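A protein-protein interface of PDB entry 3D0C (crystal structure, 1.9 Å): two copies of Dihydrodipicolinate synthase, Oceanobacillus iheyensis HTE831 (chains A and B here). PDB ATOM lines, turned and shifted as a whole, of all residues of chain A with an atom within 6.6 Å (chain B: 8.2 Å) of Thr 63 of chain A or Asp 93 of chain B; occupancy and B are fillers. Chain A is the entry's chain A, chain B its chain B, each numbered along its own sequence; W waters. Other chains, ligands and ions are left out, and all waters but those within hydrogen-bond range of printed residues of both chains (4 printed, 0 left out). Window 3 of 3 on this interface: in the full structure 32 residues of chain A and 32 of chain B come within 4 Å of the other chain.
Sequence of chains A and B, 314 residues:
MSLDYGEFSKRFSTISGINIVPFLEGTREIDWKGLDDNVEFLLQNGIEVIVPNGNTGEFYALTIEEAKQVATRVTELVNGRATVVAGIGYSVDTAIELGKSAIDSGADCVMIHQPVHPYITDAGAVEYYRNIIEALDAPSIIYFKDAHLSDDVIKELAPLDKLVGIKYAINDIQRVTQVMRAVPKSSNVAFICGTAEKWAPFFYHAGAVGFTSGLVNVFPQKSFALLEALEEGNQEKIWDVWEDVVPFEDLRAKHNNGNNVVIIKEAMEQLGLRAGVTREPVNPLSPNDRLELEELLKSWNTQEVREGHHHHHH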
ATOM      1  N   GLU A  29      11.355 -24.040  15.781  1.00  0.00           N
ATOM      2  CA  GLU A  29      11.221 -22.830  14.976  1.00  0.00           C
ATOM      3  C   GLU A  29      12.301 -22.868  13.904  1.00  0.00           C
ATOM      4  O   GLU A  29      13.304 -23.569  14.048  1.00  0.00           O
ATOM      5  CB  GLU A  29      11.383 -21.572  15.835  1.00  0.00           C
ATOM      6  CG  GLU A  29      10.253 -21.328  16.835  1.00  0.00           C
ATOM      7  CD  GLU A  29       8.885 -21.216  16.172  1.00  0.00           C
ATOM      8  OE1 GLU A  29       8.705 -20.337  15.299  1.00  0.00           O
ATOM      9  OE2 GLU A  29       7.983 -22.008  16.529  1.00  0.00           O
ATOM     10  N   PHE A  59       8.283 -28.574   3.150  1.00  0.00           N
ATOM     11  CA  PHE A  59       7.262 -27.604   2.787  1.00  0.00           C
ATOM     12  C   PHE A  59       5.956 -27.814   3.543  1.00  0.00           C
ATOM     13  O   PHE A  59       5.401 -26.869   4.109  1.00  0.00           O
ATOM     14  CB  PHE A  59       6.992 -27.691   1.279  1.00  0.00           C
ATOM     15  CG  PHE A  59       5.827 -26.861   0.816  1.00  0.00           C
ATOM     16  CD1 PHE A  59       5.837 -25.481   0.960  1.00  0.00           C
ATOM     17  CD2 PHE A  59       4.725 -27.466   0.214  1.00  0.00           C
ATOM     18  CE1 PHE A  59       4.766 -24.709   0.512  1.00  0.00           C
ATOM     19  CE2 PHE A  59       3.649 -26.702  -0.238  1.00  0.00           C
ATOM     20  CZ  PHE A  59       3.670 -25.321  -0.087  1.00  0.00           C
ATOM     21  N   TYR A  60       5.463 -29.049   3.550  1.00  0.00           N
ATOM     22  CA  TYR A  60       4.200 -29.337   4.219  1.00  0.00           C
ATOM     23  C   TYR A  60       4.202 -29.255   5.750  1.00  0.00           C
ATOM     24  O   TYR A  60       3.145 -29.312   6.369  1.00  0.00           O
ATOM     25  CB  TYR A  60       3.660 -30.693   3.747  1.00  0.00           C
ATOM     26  CG  TYR A  60       3.172 -30.646   2.314  1.00  0.00           C
ATOM     27  CD1 TYR A  60       2.089 -29.839   1.953  1.00  0.00           C
ATOM     28  CD2 TYR A  60       3.810 -31.379   1.311  1.00  0.00           C
ATOM     29  CE1 TYR A  60       1.655 -29.763   0.628  1.00  0.00           C
ATOM     30  CE2 TYR A  60       3.383 -31.308  -0.017  1.00  0.00           C
ATOM     31  CZ  TYR A  60       2.308 -30.500  -0.352  1.00  0.00           C
ATOM     32  OH  TYR A  60       1.884 -30.432  -1.657  1.00  0.00           O
ATOM     33  N   ALA A  61       5.379 -29.112   6.359  1.00  0.00           N
ATOM     34  CA  ALA A  61       5.467 -28.999   7.816  1.00  0.00           C
ATOM     35  C   ALA A  61       5.510 -27.522   8.217  1.00  0.00           C
ATOM     36  O   ALA A  61       5.618 -27.185   9.406  1.00  0.00           O
ATOM     37  CB  ALA A  61       6.712 -29.709   8.325  1.00  0.00           C
ATOM     38  N   LEU A  62       5.434 -26.652   7.211  1.00  0.00           N
ATOM     39  CA  LEU A  62       5.470 -25.208   7.412  1.00  0.00           C
ATOM     40  C   LEU A  62       4.081 -24.603   7.274  1.00  0.00           C
ATOM     41  O   LEU A  62       3.260 -25.092   6.491  1.00  0.00           O
ATOM     42  CB  LEU A  62       6.380 -24.553   6.366  1.00  0.00           C
ATOM     43  CG  LEU A  62       7.817 -25.057   6.203  1.00  0.00           C
ATOM     44  CD1 LEU A  62       8.488 -24.292   5.081  1.00  0.00           C
ATOM     45  CD2 LEU A  62       8.588 -24.877   7.509  1.00  0.00           C
ATOM     46  N   THR A  63       3.813 -23.549   8.041  1.00  0.00           N
ATOM     47  CA  THR A  63       2.533 -22.861   7.935  1.00  0.00           C
ATOM     48  C   THR A  63       2.690 -22.058   6.649  1.00  0.00           C
ATOM     49  O   THR A  63       3.792 -21.982   6.097  1.00  0.00           O
ATOM     50  CB  THR A  63       2.293 -21.860   9.091  1.00  0.00           C
ATOM     51  OG1 THR A  63       3.330 -20.874   9.085  1.00  0.00           O
ATOM     52  CG2 THR A  63       2.264 -22.570  10.439  1.00  0.00           C
ATOM     53  N   ILE A  64       1.601 -21.467   6.172  1.00  0.00           N
ATOM     54  CA  ILE A  64       1.641 -20.659   4.953  1.00  0.00           C
ATOM     55  C   ILE A  64       2.576 -19.466   5.166  1.00  0.00           C
ATOM     56  O   ILE A  64       3.383 -19.112   4.294  1.00  0.00           O
ATOM     57  CB  ILE A  64       0.214 -20.158   4.588  1.00  0.00           C
ATOM     58  CG1 ILE A  64      -0.656 -21.340   4.148  1.00  0.00           C
ATOM     59  CG2 ILE A  64       0.279 -19.091   3.497  1.00  0.00           C
ATOM     60  CD1 ILE A  64      -0.132 -22.096   2.931  1.00  0.00           C
ATOM     61  N   GLU A  65       2.468 -18.844   6.333  1.00  0.00           N
ATOM     62  CA  GLU A  65       3.312 -17.700   6.658  1.00  0.00           C
ATOM     63  C   GLU A  65       4.802 -18.071   6.629  1.00  0.00           C
ATOM     64  O   GLU A  65       5.627 -17.336   6.077  1.00  0.00           O
ATOM     65  CB  GLU A  65       2.937 -17.168   8.036  1.00  0.00           C
ATOM     66  CG  GLU A  65       3.798 -16.032   8.521  1.00  0.00           C
ATOM     67  CD  GLU A  65       3.479 -15.674   9.956  1.00  0.00           C
ATOM     68  OE1 GLU A  65       3.605 -16.567  10.823  1.00  0.00           O
ATOM     69  OE2 GLU A  65       3.101 -14.512  10.221  1.00  0.00           O
ATOM     70  N   GLU A  66       5.144 -19.205   7.234  1.00  0.00           N
ATOM     71  CA  GLU A  66       6.531 -19.652   7.251  1.00  0.00           C
ATOM     72  C   GLU A  66       7.019 -19.983   5.846  1.00  0.00           C
ATOM     73  O   GLU A  66       8.168 -19.716   5.512  1.00  0.00           O
ATOM     74  CB  GLU A  66       6.696 -20.890   8.137  1.00  0.00           C
ATOM     75  CG  GLU A  66       6.364 -20.683   9.598  1.00  0.00           C
ATOM     76  CD  GLU A  66       6.545 -21.956  10.394  1.00  0.00           C
ATOM     77  OE1 GLU A  66       5.945 -22.983  10.010  1.00  0.00           O
ATOM     78  OE2 GLU A  66       7.287 -21.935  11.396  1.00  0.00           O
ATOM     79  N   ALA A  67       6.158 -20.566   5.019  1.00  0.00           N
ATOM     80  CA  ALA A  67       6.563 -20.916   3.660  1.00  0.00           C
ATOM     81  C   ALA A  67       6.910 -19.664   2.859  1.00  0.00           C
ATOM     82  O   ALA A  67       7.900 -19.638   2.125  1.00  0.00           O
ATOM     83  CB  ALA A  67       5.456 -21.715   2.959  1.00  0.00           C
ATOM     84  N   LYS A  68       6.108 -18.615   2.993  1.00  0.00           N
ATOM     85  CA  LYS A  68       6.406 -17.385   2.275  1.00  0.00           C
ATOM     86  C   LYS A  68       7.744 -16.828   2.775  1.00  0.00           C
ATOM     87  O   LYS A  68       8.560 -16.351   1.982  1.00  0.00           O
ATOM     88  CB  LYS A  68       5.301 -16.353   2.501  1.00  0.00           C
ATOM     89  CG  LYS A  68       3.949 -16.767   1.948  1.00  0.00           C
ATOM     90  CD  LYS A  68       2.892 -15.750   2.319  1.00  0.00           C
ATOM     91  CE  LYS A  68       1.547 -16.112   1.720  1.00  0.00           C
ATOM     92  NZ  LYS A  68       0.484 -15.189   2.200  1.00  0.00           N
ATOM     93  N   GLN A  69       7.967 -16.897   4.087  1.00  0.00           N
ATOM     94  CA  GLN A  69       9.211 -16.390   4.671  1.00  0.00           C
ATOM     95  C   GLN A  69      10.444 -17.135   4.149  1.00  0.00           C
ATOM     96  O   GLN A  69      11.481 -16.523   3.893  1.00  0.00           O
ATOM     97  CB  GLN A  69       9.169 -16.480   6.199  1.00  0.00           C
ATOM     98  CG  GLN A  69       8.093 -15.622   6.853  1.00  0.00           C
ATOM     99  CD  GLN A  69       8.216 -15.585   8.367  1.00  0.00           C
ATOM    100  OE1 GLN A  69       8.286 -16.626   9.027  1.00  0.00           O
ATOM    101  NE2 GLN A  69       8.237 -14.382   8.927  1.00  0.00           N
ATOM    102  N   TYR A  90      -1.381 -26.682  -2.497  1.00  0.00           N
ATOM    103  CA  TYR A  90      -2.675 -26.521  -1.852  1.00  0.00           C
ATOM    104  C   TYR A  90      -3.771 -26.151  -2.854  1.00  0.00           C
ATOM    105  O   TYR A  90      -3.653 -26.455  -4.048  1.00  0.00           O
ATOM    106  CB  TYR A  90      -2.567 -25.483  -0.724  1.00  0.00           C
ATOM    107  CG  TYR A  90      -1.531 -25.842   0.336  1.00  0.00           C
ATOM    108  CD1 TYR A  90      -1.623 -27.037   1.052  1.00  0.00           C
ATOM    109  CD2 TYR A  90      -0.470 -24.976   0.640  1.00  0.00           C
ATOM    110  CE1 TYR A  90      -0.687 -27.367   2.052  1.00  0.00           C
ATOM    111  CE2 TYR A  90       0.470 -25.295   1.638  1.00  0.00           C
ATOM    112  CZ  TYR A  90       0.354 -26.488   2.339  1.00  0.00           C
ATOM    113  OH  TYR A  90       1.263 -26.787   3.335  1.00  0.00           O
ATOM    114  N   LEU A  98       0.684 -18.170  -2.691  1.00  0.00           N
ATOM    115  CA  LEU A  98       2.083 -18.497  -2.437  1.00  0.00           C
ATOM    116  C   LEU A  98       2.940 -18.074  -3.623  1.00  0.00           C
ATOM    117  O   LEU A  98       4.046 -17.565  -3.450  1.00  0.00           O
ATOM    118  CB  LEU A  98       2.250 -19.999  -2.201  1.00  0.00           C
ATOM    119  CG  LEU A  98       1.782 -20.563  -0.858  1.00  0.00           C
ATOM    120  CD1 LEU A  98       1.756 -22.075  -0.911  1.00  0.00           C
ATOM    121  CD2 LEU A  98       2.716 -20.090   0.236  1.00  0.00           C
ATOM    122  N   ARG A 279      10.745 -31.903  11.424  1.00  0.00           N
ATOM    123  CA  ARG A 279       9.502 -31.602  12.132  1.00  0.00           C
ATOM    124  C   ARG A 279       8.571 -32.801  12.005  1.00  0.00           C
ATOM    125  O   ARG A 279       8.823 -33.709  11.206  1.00  0.00           O
ATOM    126  CB  ARG A 279       8.801 -30.384  11.529  1.00  0.00           C
ATOM    127  CG  ARG A 279       9.310 -29.042  12.019  1.00  0.00           C
ATOM    128  CD  ARG A 279       8.393 -27.912  11.571  1.00  0.00           C
ATOM    129  NE  ARG A 279       8.838 -26.622  12.086  1.00  0.00           N
ATOM    130  CZ  ARG A 279       8.224 -25.466  11.857  1.00  0.00           C
ATOM    131  NH1 ARG A 279       7.126 -25.425  11.114  1.00  0.00           N
ATOM    132  NH2 ARG A 279       8.710 -24.347  12.377  1.00  0.00           N
ATOM    133  N   GLY B  89      -6.194 -30.407   9.277  1.00  0.00           N
ATOM    134  CA  GLY B  89      -5.016 -31.047   8.717  1.00  0.00           C
ATOM    135  C   GLY B  89      -3.891 -30.057   8.491  1.00  0.00           C
ATOM    136  O   GLY B  89      -3.879 -28.974   9.089  1.00  0.00           O
ATOM    137  N   TYR B  90      -2.949 -30.437   7.628  1.00  0.00           N
ATOM    138  CA  TYR B  90      -1.789 -29.610   7.284  1.00  0.00           C
ATOM    139  C   TYR B  90      -0.721 -29.674   8.377  1.00  0.00           C
ATOM    140  O   TYR B  90      -0.660 -30.649   9.123  1.00  0.00           O
ATOM    141  CB  TYR B  90      -2.214 -28.161   7.032  1.00  0.00           C
ATOM    142  CG  TYR B  90      -3.220 -28.017   5.913  1.00  0.00           C
ATOM    143  CD1 TYR B  90      -2.956 -28.525   4.638  1.00  0.00           C
ATOM    144  CD2 TYR B  90      -4.442 -27.377   6.126  1.00  0.00           C
ATOM    145  CE1 TYR B  90      -3.890 -28.400   3.601  1.00  0.00           C
ATOM    146  CE2 TYR B  90      -5.379 -27.246   5.103  1.00  0.00           C
ATOM    147  CZ  TYR B  90      -5.101 -27.757   3.844  1.00  0.00           C
ATOM    148  OH  TYR B  90      -6.034 -27.623   2.838  1.00  0.00           O
ATOM    149  N   SER B  91       0.123 -28.650   8.472  1.00  0.00           N
ATOM    150  CA  SER B  91       1.180 -28.663   9.486  1.00  0.00           C
ATOM    151  C   SER B  91       0.593 -28.679  10.896  1.00  0.00           C
ATOM    152  O   SER B  91      -0.590 -28.420  11.087  1.00  0.00           O
ATOM    153  CB  SER B  91       2.107 -27.454   9.328  1.00  0.00           C
ATOM    154  OG  SER B  91       1.513 -26.269   9.831  1.00  0.00           O
ATOM    155  N   VAL B  92       1.427 -28.971  11.884  1.00  0.00           N
ATOM    156  CA  VAL B  92       0.959 -29.031  13.263  1.00  0.00           C
ATOM    157  C   VAL B  92       0.263 -27.763  13.738  1.00  0.00           C
ATOM    158  O   VAL B  92      -0.825 -27.826  14.302  1.00  0.00           O
ATOM    159  CB  VAL B  92       2.113 -29.347  14.237  1.00  0.00           C
ATOM    160  CG1 VAL B  92       1.661 -29.104  15.674  1.00  0.00           C
ATOM    161  CG2 VAL B  92       2.546 -30.787  14.071  1.00  0.00           C
ATOM    162  N   ASP B  93       0.882 -26.613  13.516  1.00  0.00           N
ATOM    163  CA  ASP B  93       0.283 -25.363  13.963  1.00  0.00           C
ATOM    164  C   ASP B  93      -0.950 -24.974  13.151  1.00  0.00           C
ATOM    165  O   ASP B  93      -1.859 -24.324  13.664  1.00  0.00           O
ATOM    166  CB  ASP B  93       1.318 -24.241  13.926  1.00  0.00           C
ATOM    167  CG  ASP B  93       2.467 -24.488  14.877  1.00  0.00           C
ATOM    168  OD1 ASP B  93       2.198 -24.787  16.056  1.00  0.00           O
ATOM    169  OD2 ASP B  93       3.639 -24.391  14.448  1.00  0.00           O
ATOM    170  N   THR B  94      -0.987 -25.370  11.884  1.00  0.00           N
ATOM    171  CA  THR B  94      -2.141 -25.045  11.053  1.00  0.00           C
ATOM    172  C   THR B  94      -3.341 -25.899  11.454  1.00  0.00           C
ATOM    173  O   THR B  94      -4.481 -25.429  11.436  1.00  0.00           O
ATOM    174  CB  THR B  94      -1.860 -25.279   9.559  1.00  0.00           C
ATOM    175  OG1 THR B  94      -0.748 -24.483   9.152  1.00  0.00           O
ATOM    176  CG2 THR B  94      -3.079 -24.895   8.727  1.00  0.00           C
ATOM    177  N   ALA B  95      -3.086 -27.157  11.801  1.00  0.00           N
ATOM    178  CA  ALA B  95      -4.160 -28.052  12.212  1.00  0.00           C
ATOM    179  C   ALA B  95      -4.758 -27.518  13.512  1.00  0.00           C
ATOM    180  O   ALA B  95      -5.978 -27.515  13.698  1.00  0.00           O
ATOM    181  CB  ALA B  95      -3.621 -29.470  12.426  1.00  0.00           C
ATOM    182  N   ILE B  96      -3.881 -27.079  14.413  1.00  0.00           N
ATOM    183  CA  ILE B  96      -4.315 -26.534  15.692  1.00  0.00           C
ATOM    184  C   ILE B  96      -5.115 -25.255  15.468  1.00  0.00           C
ATOM    185  O   ILE B  96      -6.126 -25.024  16.128  1.00  0.00           O
ATOM    186  CB  ILE B  96      -3.102 -26.251  16.615  1.00  0.00           C
ATOM    187  CG1 ILE B  96      -2.420 -27.575  16.978  1.00  0.00           C
ATOM    188  CG2 ILE B  96      -3.564 -25.501  17.869  1.00  0.00           C
ATOM    189  CD1 ILE B  96      -1.130 -27.438  17.784  1.00  0.00           C
ATOM    190  N   GLU B  97      -4.671 -24.428  14.528  1.00  0.00           N
ATOM    191  CA  GLU B  97      -5.378 -23.187  14.227  1.00  0.00           C
ATOM    192  C   GLU B  97      -6.801 -23.498  13.753  1.00  0.00           C
ATOM    193  O   GLU B  97      -7.762 -22.851  14.180  1.00  0.00           O
ATOM    194  CB  GLU B  97      -4.636 -22.407  13.144  1.00  0.00           C
ATOM    195  CG  GLU B  97      -5.283 -21.086  12.779  1.00  0.00           C
ATOM    196  CD  GLU B  97      -4.603 -20.421  11.599  1.00  0.00           C
ATOM    197  OE1 GLU B  97      -3.365 -20.529  11.486  1.00  0.00           O
ATOM    198  OE2 GLU B  97      -5.299 -19.780  10.790  1.00  0.00           O
ATOM    199  N   LEU B  98      -6.925 -24.479  12.862  1.00  0.00           N
ATOM    200  CA  LEU B  98      -8.226 -24.887  12.332  1.00  0.00           C
ATOM    201  C   LEU B  98      -9.108 -25.491  13.419  1.00  0.00           C
ATOM    202  O   LEU B  98     -10.308 -25.196  13.503  1.00  0.00           O
ATOM    203  CB  LEU B  98      -8.042 -25.905  11.202  1.00  0.00           C
ATOM    204  CG  LEU B  98      -7.650 -25.330   9.837  1.00  0.00           C
ATOM    205  CD1 LEU B  98      -7.111 -26.435   8.933  1.00  0.00           C
ATOM    206  CD2 LEU B  98      -8.864 -24.666   9.204  1.00  0.00           C
ATOM    207  N   GLY B  99      -8.508 -26.333  14.253  1.00  0.00           N
ATOM    208  CA  GLY B  99      -9.251 -26.975  15.323  1.00  0.00           C
ATOM    209  C   GLY B  99      -9.813 -25.984  16.324  1.00  0.00           C
ATOM    210  O   GLY B  99     -10.980 -26.075  16.713  1.00  0.00           O
ATOM    211  N   LYS B 100      -8.978 -25.040  16.747  1.00  0.00           N
ATOM    212  CA  LYS B 100      -9.408 -24.022  17.697  1.00  0.00           C
ATOM    213  C   LYS B 100     -10.537 -23.188  17.112  1.00  0.00           C
ATOM    214  O   LYS B 100     -11.465 -22.810  17.822  1.00  0.00           O
ATOM    215  CB  LYS B 100      -8.243 -23.102  18.067  1.00  0.00           C
ATOM    216  CG  LYS B 100      -7.153 -23.789  18.846  1.00  0.00           C
ATOM    217  CD  LYS B 100      -6.103 -22.799  19.316  1.00  0.00           C
ATOM    218  CE  LYS B 100      -5.290 -23.404  20.451  1.00  0.00           C
ATOM    219  NZ  LYS B 100      -4.328 -22.440  21.045  1.00  0.00           N
ATOM    220  N   TYR B 128       3.208 -36.102  15.816  1.00  0.00           N
ATOM    221  CA  TYR B 128       2.298 -35.240  15.073  1.00  0.00           C
ATOM    222  C   TYR B 128       0.903 -35.302  15.698  1.00  0.00           C
ATOM    223  O   TYR B 128       0.332 -34.276  16.070  1.00  0.00           O
ATOM    224  CB  TYR B 128       2.232 -35.697  13.611  1.00  0.00           C
ATOM    225  CG  TYR B 128       1.247 -34.939  12.745  1.00  0.00           C
ATOM    226  CD1 TYR B 128       1.576 -33.704  12.190  1.00  0.00           C
ATOM    227  CD2 TYR B 128      -0.016 -35.467  12.475  1.00  0.00           C
ATOM    228  CE1 TYR B 128       0.668 -33.012  11.383  1.00  0.00           C
ATOM    229  CE2 TYR B 128      -0.930 -34.784  11.675  1.00  0.00           C
ATOM    230  CZ  TYR B 128      -0.581 -33.558  11.130  1.00  0.00           C
ATOM    231  OH  TYR B 128      -1.475 -32.876  10.335  1.00  0.00           O
ATOM    232  N   ASN B 131       0.785 -34.115  19.528  1.00  0.00           N
ATOM    233  CA  ASN B 131       0.915 -32.664  19.627  1.00  0.00           C
ATOM    234  C   ASN B 131      -0.337 -31.884  19.260  1.00  0.00           C
ATOM    235  O   ASN B 131      -0.603 -30.830  19.834  1.00  0.00           O
ATOM    236  CB  ASN B 131       2.081 -32.164  18.767  1.00  0.00           C
ATOM    237  CG  ASN B 131       3.434 -32.495  19.370  1.00  0.00           C
ATOM    238  OD1 ASN B 131       3.538 -32.760  20.566  1.00  0.00           O
ATOM    239  ND2 ASN B 131       4.478 -32.463  18.547  1.00  0.00           N
ATOM    240  N   ILE B 132      -1.101 -32.389  18.301  1.00  0.00           N
ATOM    241  CA  ILE B 132      -2.319 -31.710  17.884  1.00  0.00           C
ATOM    242  C   ILE B 132      -3.432 -31.993  18.893  1.00  0.00           C
ATOM    243  O   ILE B 132      -4.118 -31.077  19.354  1.00  0.00           O
ATOM    244  CB  ILE B 132      -2.762 -32.178  16.467  1.00  0.00           C
ATOM    245  CG1 ILE B 132      -1.721 -31.750  15.425  1.00  0.00           C
ATOM    246  CG2 ILE B 132      -4.129 -31.595  16.121  1.00  0.00           C
ATOM    247  CD1 ILE B 132      -1.993 -32.287  14.030  1.00  0.00           C
ATOM    248  N   ALA B 135      -3.053 -30.119  22.193  1.00  0.00           N
ATOM    249  CA  ALA B 135      -3.259 -28.677  22.086  1.00  0.00           C
ATOM    250  C   ALA B 135      -4.721 -28.258  21.902  1.00  0.00           C
ATOM    251  O   ALA B 135      -5.049 -27.082  22.046  1.00  0.00           O
ATOM    252  CB  ALA B 135      -2.402 -28.103  20.948  1.00  0.00           C
ATOM    253  N   LEU B 136      -5.596 -29.207  21.588  1.00  0.00           N
ATOM    254  CA  LEU B 136      -7.007 -28.890  21.390  1.00  0.00           C
ATOM    255  C   LEU B 136      -7.872 -29.274  22.584  1.00  0.00           C
ATOM    256  O   LEU B 136      -7.786 -30.389  23.098  1.00  0.00           O
ATOM    257  CB  LEU B 136      -7.539 -29.587  20.137  1.00  0.00           C
ATOM    258  CG  LEU B 136      -6.872 -29.198  18.814  1.00  0.00           C
ATOM    259  CD1 LEU B 136      -7.429 -30.055  17.687  1.00  0.00           C
ATOM    260  CD2 LEU B 136      -7.099 -27.715  18.541  1.00  0.00           C
HETATM  261  O   HOH W   1       4.560 -28.471  11.468  1.00  0.00           O
HETATM  262  O   HOH W   2       0.630 -28.707   5.231  1.00  0.00           O
HETATM  263  O   HOH W   3      -0.983 -22.482   7.206  1.00  0.00           O
HETATM  264  O   HOH W   4       0.677 -26.032   7.056  1.00  0.00           O
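Water W1 bridges the backbone carbonyl oxygen (O) of Ala 61 of chain A (2.7 Å) and the backbone NH (N) of Val 92 of chain B (3.2 Å).
Water W2 lies within hydrogen-bond range of the side-chain hydroxyl (OH) of Tyr 90 of chain A, the backbone carbonyl oxygen (O) of Tyr 60 of chain A and the backbone NH (N) of Ser 91 of chain B.
Water W3 bridges OG1 of Thr 94 of chain B and N of Ile 64 of chain A.
Water W4 lies within hydrogen-bond range of O of Leu 62 of chain A, OG of Ser 91 of chain B and OG1 of Thr 94 of chain B.
Of the printed residues of chain B, Thr 63 of chain A touches Ser 91 (3.8 Å), Asp 93 (3.98 Å) and Thr 94 (3.8 Å).
Of the printed residues of chain A, Asp 93 of chain B touches Thr 63.
Of the printed residues of chain A, Ser 91 of chain B touches Tyr 60 (3.6 Å), Ala 61 (3.5 Å), Leu 62 (3.9 Å) and Thr 63 (3.8 Å).
Of the printed residues of chain B, Ala 61 of chain A touches Ser 91.
Of the printed residues of chain A, Thr 94 of chain B touches Thr 63.
Phe 59 of chain A touches none of the printed residues of chain B.
The nearest printed residue of chain B that does not touch Thr 63 of chain A is Glu 97 of chain B (6.1 Å).
The nearest printed residue of chain B that does not touch Tyr 90 of chain A is Ser 91 of chain B (5.6 Å).
Of the 15 printed residues of chain A, 5 touch a printed residue of chain B.
Hydrophobic or aromatic side chains of chain A within 4 Å of the printed part of chain B: Tyr 90.
Among the printed residues, 7 pairs touch across the chains.
Among the printed residues, no Asp or Glu carboxylate lies within 4 Å of a Lys or Arg side-chain nitrogen of the other chain.
Ser 91 of chain B touches Tyr 60 of chain A (CB to O, 3.6 Å).
Ser 91 of chain B touches Ala 61 of chain A (CB to O, 3.5 Å).
O of Leu 62 of chain A touches CB of Ser 91 of chain B, 3.9 Å away.
CG2 of Thr 63 of chain A touches OG of Ser 91 of chain B (3.8 Å).
Thr 63 of chain A touches Asp 93 of chain B (CG2 to CB, 3.98 Å).
Thr 63 of chain A touches Thr 94 of chain B (CG2 to OG1, 3.8 Å).
Tyr 90 of chain A touches Tyr 90 of chain B.
The backbone carbonyl oxygen (O) of Ala 61 of chain A lies within hydrogen-bond range of the guanidinium group (NH1) of Arg 279 of chain A.
The backbone NH (N) of Thr 63 of chain A lies within hydrogen-bond range of the side-chain carboxylate (OE1) of Glu 66 of chain A (3.0 Å).
OH of Tyr 128 of chain B is in hydrogen-bond range of O of Tyr 90 of chain B, 2.7 Å away.
OG of Ser 91 of chain B lies within hydrogen-bond range of OG1 of Thr 94 of chain B (3.0 Å).
Tyr 90 of chain A touches its own counterpart, Tyr 90 of chain B.
Positions printed for both chains: 90 and 98.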
